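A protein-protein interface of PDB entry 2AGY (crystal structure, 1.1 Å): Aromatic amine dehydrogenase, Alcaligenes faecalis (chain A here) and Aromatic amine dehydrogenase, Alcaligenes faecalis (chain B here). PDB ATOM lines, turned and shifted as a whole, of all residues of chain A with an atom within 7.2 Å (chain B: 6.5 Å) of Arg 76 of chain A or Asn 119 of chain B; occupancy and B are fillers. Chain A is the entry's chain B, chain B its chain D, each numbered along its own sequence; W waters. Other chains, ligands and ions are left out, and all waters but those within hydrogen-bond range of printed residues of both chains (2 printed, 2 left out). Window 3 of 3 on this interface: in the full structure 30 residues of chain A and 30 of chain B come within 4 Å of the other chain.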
ATOM      1  N   THR A  69     -19.511  14.438   8.835  1.00  0.00           N
ATOM      2  CA  THR A  69     -19.022  13.407   9.728  1.00  0.00           C
ATOM      3  C   THR A  69     -17.541  13.575   9.914  1.00  0.00           C
ATOM      4  O   THR A  69     -16.794  13.714   8.938  1.00  0.00           O
ATOM      5  CB  THR A  69     -19.287  12.022   9.120  1.00  0.00           C
ATOM      6  OG1 THR A  69     -20.696  11.785   9.053  1.00  0.00           O
ATOM      7  CG2 THR A  69     -18.663  10.897   9.966  1.00  0.00           C
ATOM      8  N   TYR A  70     -17.128  13.533  11.171  1.00  0.00           N
ATOM      9  CA  TYR A  70     -15.744  13.471  11.556  1.00  0.00           C
ATOM     10  C   TYR A  70     -15.479  12.148  12.262  1.00  0.00           C
ATOM     11  O   TYR A  70     -16.397  11.525  12.829  1.00  0.00           O
ATOM     12  CB  TYR A  70     -15.413  14.563  12.539  1.00  0.00           C
ATOM     13  CG  TYR A  70     -15.589  15.969  12.028  1.00  0.00           C
ATOM     14  CD1 TYR A  70     -16.762  16.671  12.256  1.00  0.00           C
ATOM     15  CD2 TYR A  70     -14.593  16.589  11.331  1.00  0.00           C
ATOM     16  CE1 TYR A  70     -16.923  17.971  11.800  1.00  0.00           C
ATOM     17  CE2 TYR A  70     -14.742  17.894  10.870  1.00  0.00           C
ATOM     18  CZ  TYR A  70     -15.904  18.572  11.104  1.00  0.00           C
ATOM     19  OH  TYR A  70     -16.032  19.881  10.640  1.00  0.00           O
ATOM     20  N   HIS A  71     -14.228  11.721  12.247  1.00  0.00           N
ATOM     21  CA  HIS A  71     -13.756  10.711  13.193  1.00  0.00           C
ATOM     22  C   HIS A  71     -12.452  11.208  13.799  1.00  0.00           C
ATOM     23  O   HIS A  71     -11.701  11.978  13.180  1.00  0.00           O
ATOM     24  CB  HIS A  71     -13.507   9.348  12.543  1.00  0.00           C
ATOM     25  CG  HIS A  71     -14.711   8.712  11.945  1.00  0.00           C
ATOM     26  ND1 HIS A  71     -15.425   7.701  12.562  1.00  0.00           N
ATOM     27  CD2 HIS A  71     -15.315   8.931  10.764  1.00  0.00           C
ATOM     28  CE1 HIS A  71     -16.426   7.333  11.772  1.00  0.00           C
ATOM     29  NE2 HIS A  71     -16.383   8.069  10.680  1.00  0.00           N
ATOM     30  N   GLU A  72     -12.157  10.743  15.016  1.00  0.00           N
ATOM     31  CA  GLU A  72     -10.984  11.253  15.736  1.00  0.00           C
ATOM     32  C   GLU A  72      -9.696  11.122  14.945  1.00  0.00           C
ATOM     33  O   GLU A  72      -8.802  11.962  15.053  1.00  0.00           O
ATOM     34  CB  GLU A  72     -10.800  10.516  17.054  1.00  0.00           C
ATOM     35  CG  GLU A  72     -11.929  10.603  18.047  1.00  0.00           C
ATOM     36  CD  GLU A  72     -11.699   9.703  19.280  1.00  0.00           C
ATOM     37  OE1 GLU A  72     -11.588   8.430  19.136  1.00  0.00           O
ATOM     38  OE2 GLU A  72     -11.631  10.258  20.401  1.00  0.00           O
ATOM     39  N   ARG A  73      -9.589  10.046  14.156  1.00  0.00           N
ATOM     40  CA  ARG A  73      -8.428   9.827  13.328  1.00  0.00           C
ATOM     41  C   ARG A  73      -8.838   9.538  11.876  1.00  0.00           C
ATOM     42  O   ARG A  73      -8.142   8.836  11.154  1.00  0.00           O
ATOM     43  CB  ARG A  73      -7.574   8.706  13.914  1.00  0.00           C
ATOM     44  CG  ARG A  73      -6.935   9.085  15.217  1.00  0.00           C
ATOM     45  CD  ARG A  73      -5.763  10.008  15.038  1.00  0.00           C
ATOM     46  NE  ARG A  73      -5.050  10.266  16.283  1.00  0.00           N
ATOM     47  CZ  ARG A  73      -5.337  11.203  17.138  1.00  0.00           C
ATOM     48  NH1 ARG A  73      -6.322  12.037  16.921  1.00  0.00           N
ATOM     49  NH2 ARG A  73      -4.610  11.317  18.237  1.00  0.00           N
ATOM     50  N   ILE A  74      -9.979  10.117  11.483  1.00  0.00           N
ATOM     51  CA  ILE A  74     -10.515  10.107  10.110  1.00  0.00           C
ATOM     52  C   ILE A  74     -11.017   8.743   9.688  1.00  0.00           C
ATOM     53  O   ILE A  74     -12.216   8.554   9.502  1.00  0.00           O
ATOM     54  CB  ILE A  74      -9.526  10.663   9.079  1.00  0.00           C
ATOM     55  CG1 ILE A  74      -8.994  12.032   9.504  1.00  0.00           C
ATOM     56  CG2 ILE A  74     -10.212  10.754   7.703  1.00  0.00           C
ATOM     57  CD1 ILE A  74      -7.877  12.510   8.683  1.00  0.00           C
ATOM     58  N   THR A  75     -10.089   7.808   9.521  1.00  0.00           N
ATOM     59  CA  THR A  75     -10.398   6.446   9.137  1.00  0.00           C
ATOM     60  C   THR A  75     -10.473   5.462  10.312  1.00  0.00           C
ATOM     61  O   THR A  75     -10.694   4.293  10.111  1.00  0.00           O
ATOM     62  CB  THR A  75      -9.370   5.949   8.134  1.00  0.00           C
ATOM     63  OG1 THR A  75      -8.057   6.296   8.568  1.00  0.00           O
ATOM     64  CG2 THR A  75      -9.550   6.638   6.781  1.00  0.00           C
ATOM     65  N   ARG A  76     -10.277   5.968  11.525  1.00  0.00           N
ATOM     66  CA  ARG A  76     -10.498   5.208  12.733  1.00  0.00           C
ATOM     67  C   ARG A  76     -10.862   6.199  13.831  1.00  0.00           C
ATOM     68  O   ARG A  76     -10.755   7.418  13.656  1.00  0.00           O
ATOM     69  CB  ARG A  76      -9.253   4.388  13.110  1.00  0.00           C
ATOM     70  CG  ARG A  76      -8.033   5.215  13.412  1.00  0.00           C
ATOM     71  CD  ARG A  76      -6.740   4.391  13.594  1.00  0.00           C
ATOM     72  NE  ARG A  76      -5.610   5.275  13.677  1.00  0.00           N
ATOM     73  CZ  ARG A  76      -5.193   5.863  14.775  1.00  0.00           C
ATOM     74  NH1 ARG A  76      -5.779   5.635  15.924  1.00  0.00           N
ATOM     75  NH2 ARG A  76      -4.159   6.691  14.716  1.00  0.00           N
ATOM     76  N   GLY A  77     -11.293   5.671  14.954  1.00  0.00           N
ATOM     77  CA  GLY A  77     -11.655   6.494  16.090  1.00  0.00           C
ATOM     78  C   GLY A  77     -13.119   6.859  16.105  1.00  0.00           C
ATOM     79  O   GLY A  77     -13.874   6.535  15.198  1.00  0.00           O
ATOM     80  N   LYS A  78     -13.511   7.557  17.162  1.00  0.00           N
ATOM     81  CA  LYS A  78     -14.904   7.842  17.404  1.00  0.00           C
ATOM     82  C   LYS A  78     -15.494   8.765  16.350  1.00  0.00           C
ATOM     83  O   LYS A  78     -14.870   9.725  15.936  1.00  0.00           O
ATOM     84  CB  LYS A  78     -15.080   8.498  18.769  1.00  0.00           C
ATOM     85  CG  LYS A  78     -16.546   8.769  19.133  1.00  0.00           C
ATOM     86  CD  LYS A  78     -16.709   9.258  20.560  1.00  0.00           C
ATOM     87  CE  LYS A  78     -18.188   9.258  20.993  1.00  0.00           C
ATOM     88  NZ  LYS A  78     -18.344   9.212  22.478  1.00  0.00           N
ATOM     89  N   ARG A  79     -16.716   8.433  15.947  1.00  0.00           N
ATOM     90  CA  ARG A  79     -17.490   9.191  14.974  1.00  0.00           C
ATOM     91  C   ARG A  79     -18.215  10.353  15.622  1.00  0.00           C
ATOM     92  O   ARG A  79     -18.815  10.203  16.696  1.00  0.00           O
ATOM     93  CB  ARG A  79     -18.528   8.283  14.356  1.00  0.00           C
ATOM     94  CG  ARG A  79     -19.401   8.922  13.298  1.00  0.00           C
ATOM     95  CD  ARG A  79     -20.088   7.899  12.427  1.00  0.00           C
ATOM     96  NE  ARG A  79     -21.186   8.469  11.666  1.00  0.00           N
ATOM     97  CZ  ARG A  79     -21.920   7.777  10.827  1.00  0.00           C
ATOM     98  NH1 ARG A  79     -21.655   6.490  10.619  1.00  0.00           N
ATOM     99  NH2 ARG A  79     -22.914   8.357  10.179  1.00  0.00           N
ATOM    100  N   GLN A 105     -25.253   9.571   4.798  1.00  0.00           N
ATOM    101  CA  GLN A 105     -24.071   9.714   3.977  1.00  0.00           C
ATOM    102  C   GLN A 105     -24.475   9.295   2.594  1.00  0.00           C
ATOM    103  O   GLN A 105     -24.832   8.146   2.339  1.00  0.00           O
ATOM    104  CB  GLN A 105     -22.934   8.863   4.541  1.00  0.00           C
ATOM    105  CG  GLN A 105     -22.495   9.371   5.926  1.00  0.00           C
ATOM    106  CD  GLN A 105     -21.424   8.551   6.579  1.00  0.00           C
ATOM    107  OE1 GLN A 105     -20.776   8.997   7.544  1.00  0.00           O
ATOM    108  NE2 GLN A 105     -21.226   7.388   6.095  1.00  0.00           N
ATOM    109  N   THR B  56     -12.523  -2.853   5.500  1.00  0.00           N
ATOM    110  CA  THR B  56     -13.453  -3.701   6.238  1.00  0.00           C
ATOM    111  C   THR B  56     -14.755  -3.825   5.463  1.00  0.00           C
ATOM    112  O   THR B  56     -15.310  -2.814   5.054  1.00  0.00           O
ATOM    113  CB  THR B  56     -13.745  -3.004   7.625  1.00  0.00           C
ATOM    114  OG1 THR B  56     -12.504  -2.763   8.329  1.00  0.00           O
ATOM    115  CG2 THR B  56     -14.558  -3.884   8.535  1.00  0.00           C
ATOM    116  N   CYS B  83     -14.590  -0.513   3.661  1.00  0.00           N
ATOM    117  CA  CYS B  83     -14.697   0.688   4.474  1.00  0.00           C
ATOM    118  C   CYS B  83     -13.464   0.899   5.347  1.00  0.00           C
ATOM    119  O   CYS B  83     -12.681   0.000   5.574  1.00  0.00           O
ATOM    120  CB  CYS B  83     -15.923   0.526   5.378  1.00  0.00           C
ATOM    121  SG  CYS B  83     -17.419  -0.028   4.489  1.00  0.00           S
ATOM    122  N   GLY B  84     -13.316   2.110   5.833  1.00  0.00           N
ATOM    123  CA  GLY B  84     -12.294   2.411   6.801  1.00  0.00           C
ATOM    124  C   GLY B  84     -10.954   2.760   6.193  1.00  0.00           C
ATOM    125  O   GLY B  84      -9.961   2.789   6.899  1.00  0.00           O
ATOM    126  N   LYS B  85     -10.933   3.021   4.888  1.00  0.00           N
ATOM    127  CA  LYS B  85      -9.814   3.627   4.186  1.00  0.00           C
ATOM    128  C   LYS B  85     -10.409   4.634   3.238  1.00  0.00           C
ATOM    129  O   LYS B  85     -11.559   4.522   2.835  1.00  0.00           O
ATOM    130  CB  LYS B  85      -8.957   2.602   3.415  1.00  0.00           C
ATOM    131  CG  LYS B  85      -8.025   1.824   4.302  1.00  0.00           C
ATOM    132  CD  LYS B  85      -7.007   0.999   3.558  1.00  0.00           C
ATOM    133  CE  LYS B  85      -5.994   0.506   4.515  1.00  0.00           C
ATOM    134  NZ  LYS B  85      -5.038  -0.426   3.934  1.00  0.00           N
ATOM    135  N   CYS B 114     -21.209   1.836   3.593  1.00  0.00           N
ATOM    136  CA  CYS B 114     -20.372   1.808   4.798  1.00  0.00           C
ATOM    137  C   CYS B 114     -20.972   2.547   5.997  1.00  0.00           C
ATOM    138  O   CYS B 114     -20.331   2.651   7.025  1.00  0.00           O
ATOM    139  CB  CYS B 114     -19.023   2.461   4.509  1.00  0.00           C
ATOM    140  SG  CYS B 114     -17.945   1.589   3.395  1.00  0.00           S
ATOM    141  N   ALA B 116     -22.888   2.164   8.411  1.00  0.00           N
ATOM    142  CA  ALA B 116     -23.010   1.542   9.745  1.00  0.00           C
ATOM    143  C   ALA B 116     -21.737   0.857  10.207  1.00  0.00           C
ATOM    144  O   ALA B 116     -21.725   0.211  11.246  1.00  0.00           O
ATOM    145  CB  ALA B 116     -24.155   0.544   9.750  1.00  0.00           C
ATOM    146  N   ASN B 117     -20.656   0.984   9.444  1.00  0.00           N
ATOM    147  CA  ASN B 117     -19.382   0.408   9.845  1.00  0.00           C
ATOM    148  C   ASN B 117     -18.751   1.198  10.967  1.00  0.00           C
ATOM    149  O   ASN B 117     -19.062   2.358  11.173  1.00  0.00           O
ATOM    150  CB  ASN B 117     -18.416   0.350   8.676  1.00  0.00           C
ATOM    151  CG  ASN B 117     -18.550  -0.898   7.881  1.00  0.00           C
ATOM    152  OD1 ASN B 117     -17.587  -1.687   7.781  1.00  0.00           O
ATOM    153  ND2 ASN B 117     -19.709  -1.118   7.312  1.00  0.00           N
ATOM    154  N   GLU B 118     -17.833   0.574  11.679  1.00  0.00           N
ATOM    155  CA  GLU B 118     -17.127   1.232  12.738  1.00  0.00           C
ATOM    156  C   GLU B 118     -16.433   2.491  12.227  1.00  0.00           C
ATOM    157  O   GLU B 118     -16.402   3.511  12.918  1.00  0.00           O
ATOM    158  CB  GLU B 118     -16.103   0.281  13.371  1.00  0.00           C
ATOM    159  CG  GLU B 118     -15.248   0.951  14.432  1.00  0.00           C
ATOM    160  CD  GLU B 118     -14.607   0.003  15.404  1.00  0.00           C
ATOM    161  OE1 GLU B 118     -15.344  -0.594  16.216  1.00  0.00           O
ATOM    162  OE2 GLU B 118     -13.360  -0.141  15.362  1.00  0.00           O
ATOM    163  N   ASN B 119     -15.870   2.420  11.023  1.00  0.00           N
ATOM    164  CA  ASN B 119     -15.477   3.586  10.302  1.00  0.00           C
ATOM    165  C   ASN B 119     -16.162   3.623   8.963  1.00  0.00           C
ATOM    166  O   ASN B 119     -16.012   2.732   8.142  1.00  0.00           O
ATOM    167  CB  ASN B 119     -13.982   3.687  10.119  1.00  0.00           C
ATOM    168  CG  ASN B 119     -13.610   5.022   9.588  1.00  0.00           C
ATOM    169  OD1 ASN B 119     -13.485   5.217   8.363  1.00  0.00           O
ATOM    170  ND2 ASN B 119     -13.457   5.991  10.487  1.00  0.00           N
ATOM    171  N   SER B 120     -16.904   4.703   8.735  1.00  0.00           N
ATOM    172  CA  SER B 120     -17.757   4.814   7.564  1.00  0.00           C
ATOM    173  C   SER B 120     -17.052   5.358   6.329  1.00  0.00           C
ATOM    174  O   SER B 120     -17.689   5.534   5.308  1.00  0.00           O
ATOM    175  CB  SER B 120     -18.978   5.655   7.882  1.00  0.00           C
ATOM    176  OG  SER B 120     -18.620   6.894   8.433  1.00  0.00           O
ATOM    177  N   THR B 121     -15.753   5.633   6.394  1.00  0.00           N
ATOM    178  CA  THR B 121     -15.073   6.150   5.208  1.00  0.00           C
ATOM    179  C   THR B 121     -15.147   5.118   4.100  1.00  0.00           C
ATOM    180  O   THR B 121     -14.843   3.958   4.304  1.00  0.00           O
ATOM    181  CB  THR B 121     -13.618   6.484   5.501  1.00  0.00           C
ATOM    182  OG1 THR B 121     -13.540   7.340   6.646  1.00  0.00           O
ATOM    183  CG2 THR B 121     -12.991   7.256   4.355  1.00  0.00           C
ATOM    184  N   PHE B 122     -15.561   5.550   2.925  1.00  0.00           N
ATOM    185  CA  PHE B 122     -15.793   4.670   1.805  1.00  0.00           C
ATOM    186  C   PHE B 122     -14.521   4.435   0.993  1.00  0.00           C
ATOM    187  O   PHE B 122     -13.883   5.405   0.544  1.00  0.00           O
ATOM    188  CB  PHE B 122     -16.876   5.239   0.901  1.00  0.00           C
ATOM    189  CG  PHE B 122     -16.986   4.514  -0.395  1.00  0.00           C
ATOM    190  CD1 PHE B 122     -17.526   3.239  -0.442  1.00  0.00           C
ATOM    191  CD2 PHE B 122     -16.533   5.075  -1.560  1.00  0.00           C
ATOM    192  CE1 PHE B 122     -17.620   2.553  -1.644  1.00  0.00           C
ATOM    193  CE2 PHE B 122     -16.625   4.410  -2.754  1.00  0.00           C
ATOM    194  CZ  PHE B 122     -17.163   3.148  -2.800  1.00  0.00           C
HETATM  195  O   HOH W   1     -10.120   1.546   9.832  1.00  0.00           O
HETATM  196  O   HOH W   2     -13.880   4.816  13.151  1.00  0.00           O
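The side-chain amide nitrogen (ND2) of Asn 119 of chain B lies within hydrogen-bond range of the backbone carbonyl oxygen (O) of Ile 74 of chain A, at 3.0 Å.
OG1 of Thr 121 of chain B lies within hydrogen-bond range of O of Ile 74 of chain A.
A ring nitrogen (NE2) of His 71 of chain A lies within hydrogen-bond range of the side-chain hydroxyl (OG) of Ser 120 of chain B, 3.4 Å away.
ND2 of Asn 119 of chain B lies close to ND1 of His 71 of chain A (3.3 Å).
The side-chain amide oxygen of Gln 105 of chain A lies within hydrogen-bond range of the side-chain hydroxyl of Ser 120 of chain B, 3.1 Å away.
The side-chain amide nitrogen (ND2) of Asn 119 of chain B sits close to the backbone NH (N) of Arg 76 of chain A.
O of Thr 75 of chain A lies close to ND2 of Asn 119 of chain B (3.3 Å).
SG of Cys 83 of chain B forms a disulfide with SG of Cys 114 of chain B.
OG1 of Thr 69 of chain A sits at hydrogen-bond distance from OE1 of Gln 105 of chain A, 3.2 Å away.
ND1 of His 71 of chain A lies within hydrogen-bond range of O of Gly 77 of chain A, at 3.3 Å.
OG1 of Thr 121 of chain B lies within hydrogen-bond range of OD1 of Asn 119 of chain B.
The backbone carbonyl oxygen (O) of Thr 121 of chain B sits at hydrogen-bond distance from the backbone NH (N) of Gly 84 of chain B (2.8 Å).
NH2 of Arg 79 of chain A is in hydrogen-bond range of OE1 of Gln 105 of chain A (3.5 Å).
CE1 of His 71 of chain A touches O of Glu 118 of chain B (3.99 Å).
CB of Thr 75 of chain A touches O of Gly 84 of chain B (3.4 Å).
Lys 85 of chain B touches Thr 75 of chain A (CA to CG2, 3.98 Å).
OG of Ser 120 of chain B touches NH1 of Arg 79 of chain A, at 3.8 Å.
Of chain B, only Asn 119 (3.3 Å) comes within 4 Å of Arg 76 of chain A.
Asn 119 of chain B touches four residues of chain A.
Printed residues of chain A within 4 Å of Glu 118 of chain B: His 71.
Printed residues of chain A within 4 Å of Gly 84 of chain B: Thr 75 (3.4 Å).
The nearest residue of chain B that does not touch Arg 76 of chain A is Gly 84 of chain B (5.6 Å).
The nearest printed residue of chain B that does not touch Arg 79 of chain A is Asn 117 of chain B (4.9 Å).
Hydrophobic or aromatic side chains of chain A within 4 Å of the printed part of chain B: His 71.
Along chain A the printed residues that touch a printed residue of chain B span positions 71 to 105.
Among the printed residues, 11 pairs touch across the chains.
Water W2 lies within hydrogen-bond range of the backbone carbonyl oxygen of Gly 77 of chain A, the backbone carbonyl oxygen of Glu 118 of chain B, the side-chain amide nitrogen of Asn 119 of chain B and a ring nitrogen (ND1) of His 71 of chain A.
Water W1 bridges the backbone carbonyl oxygen (O) of Thr 75 of chain A and the backbone carbonyl oxygen (O) of Gly 84 of chain B.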
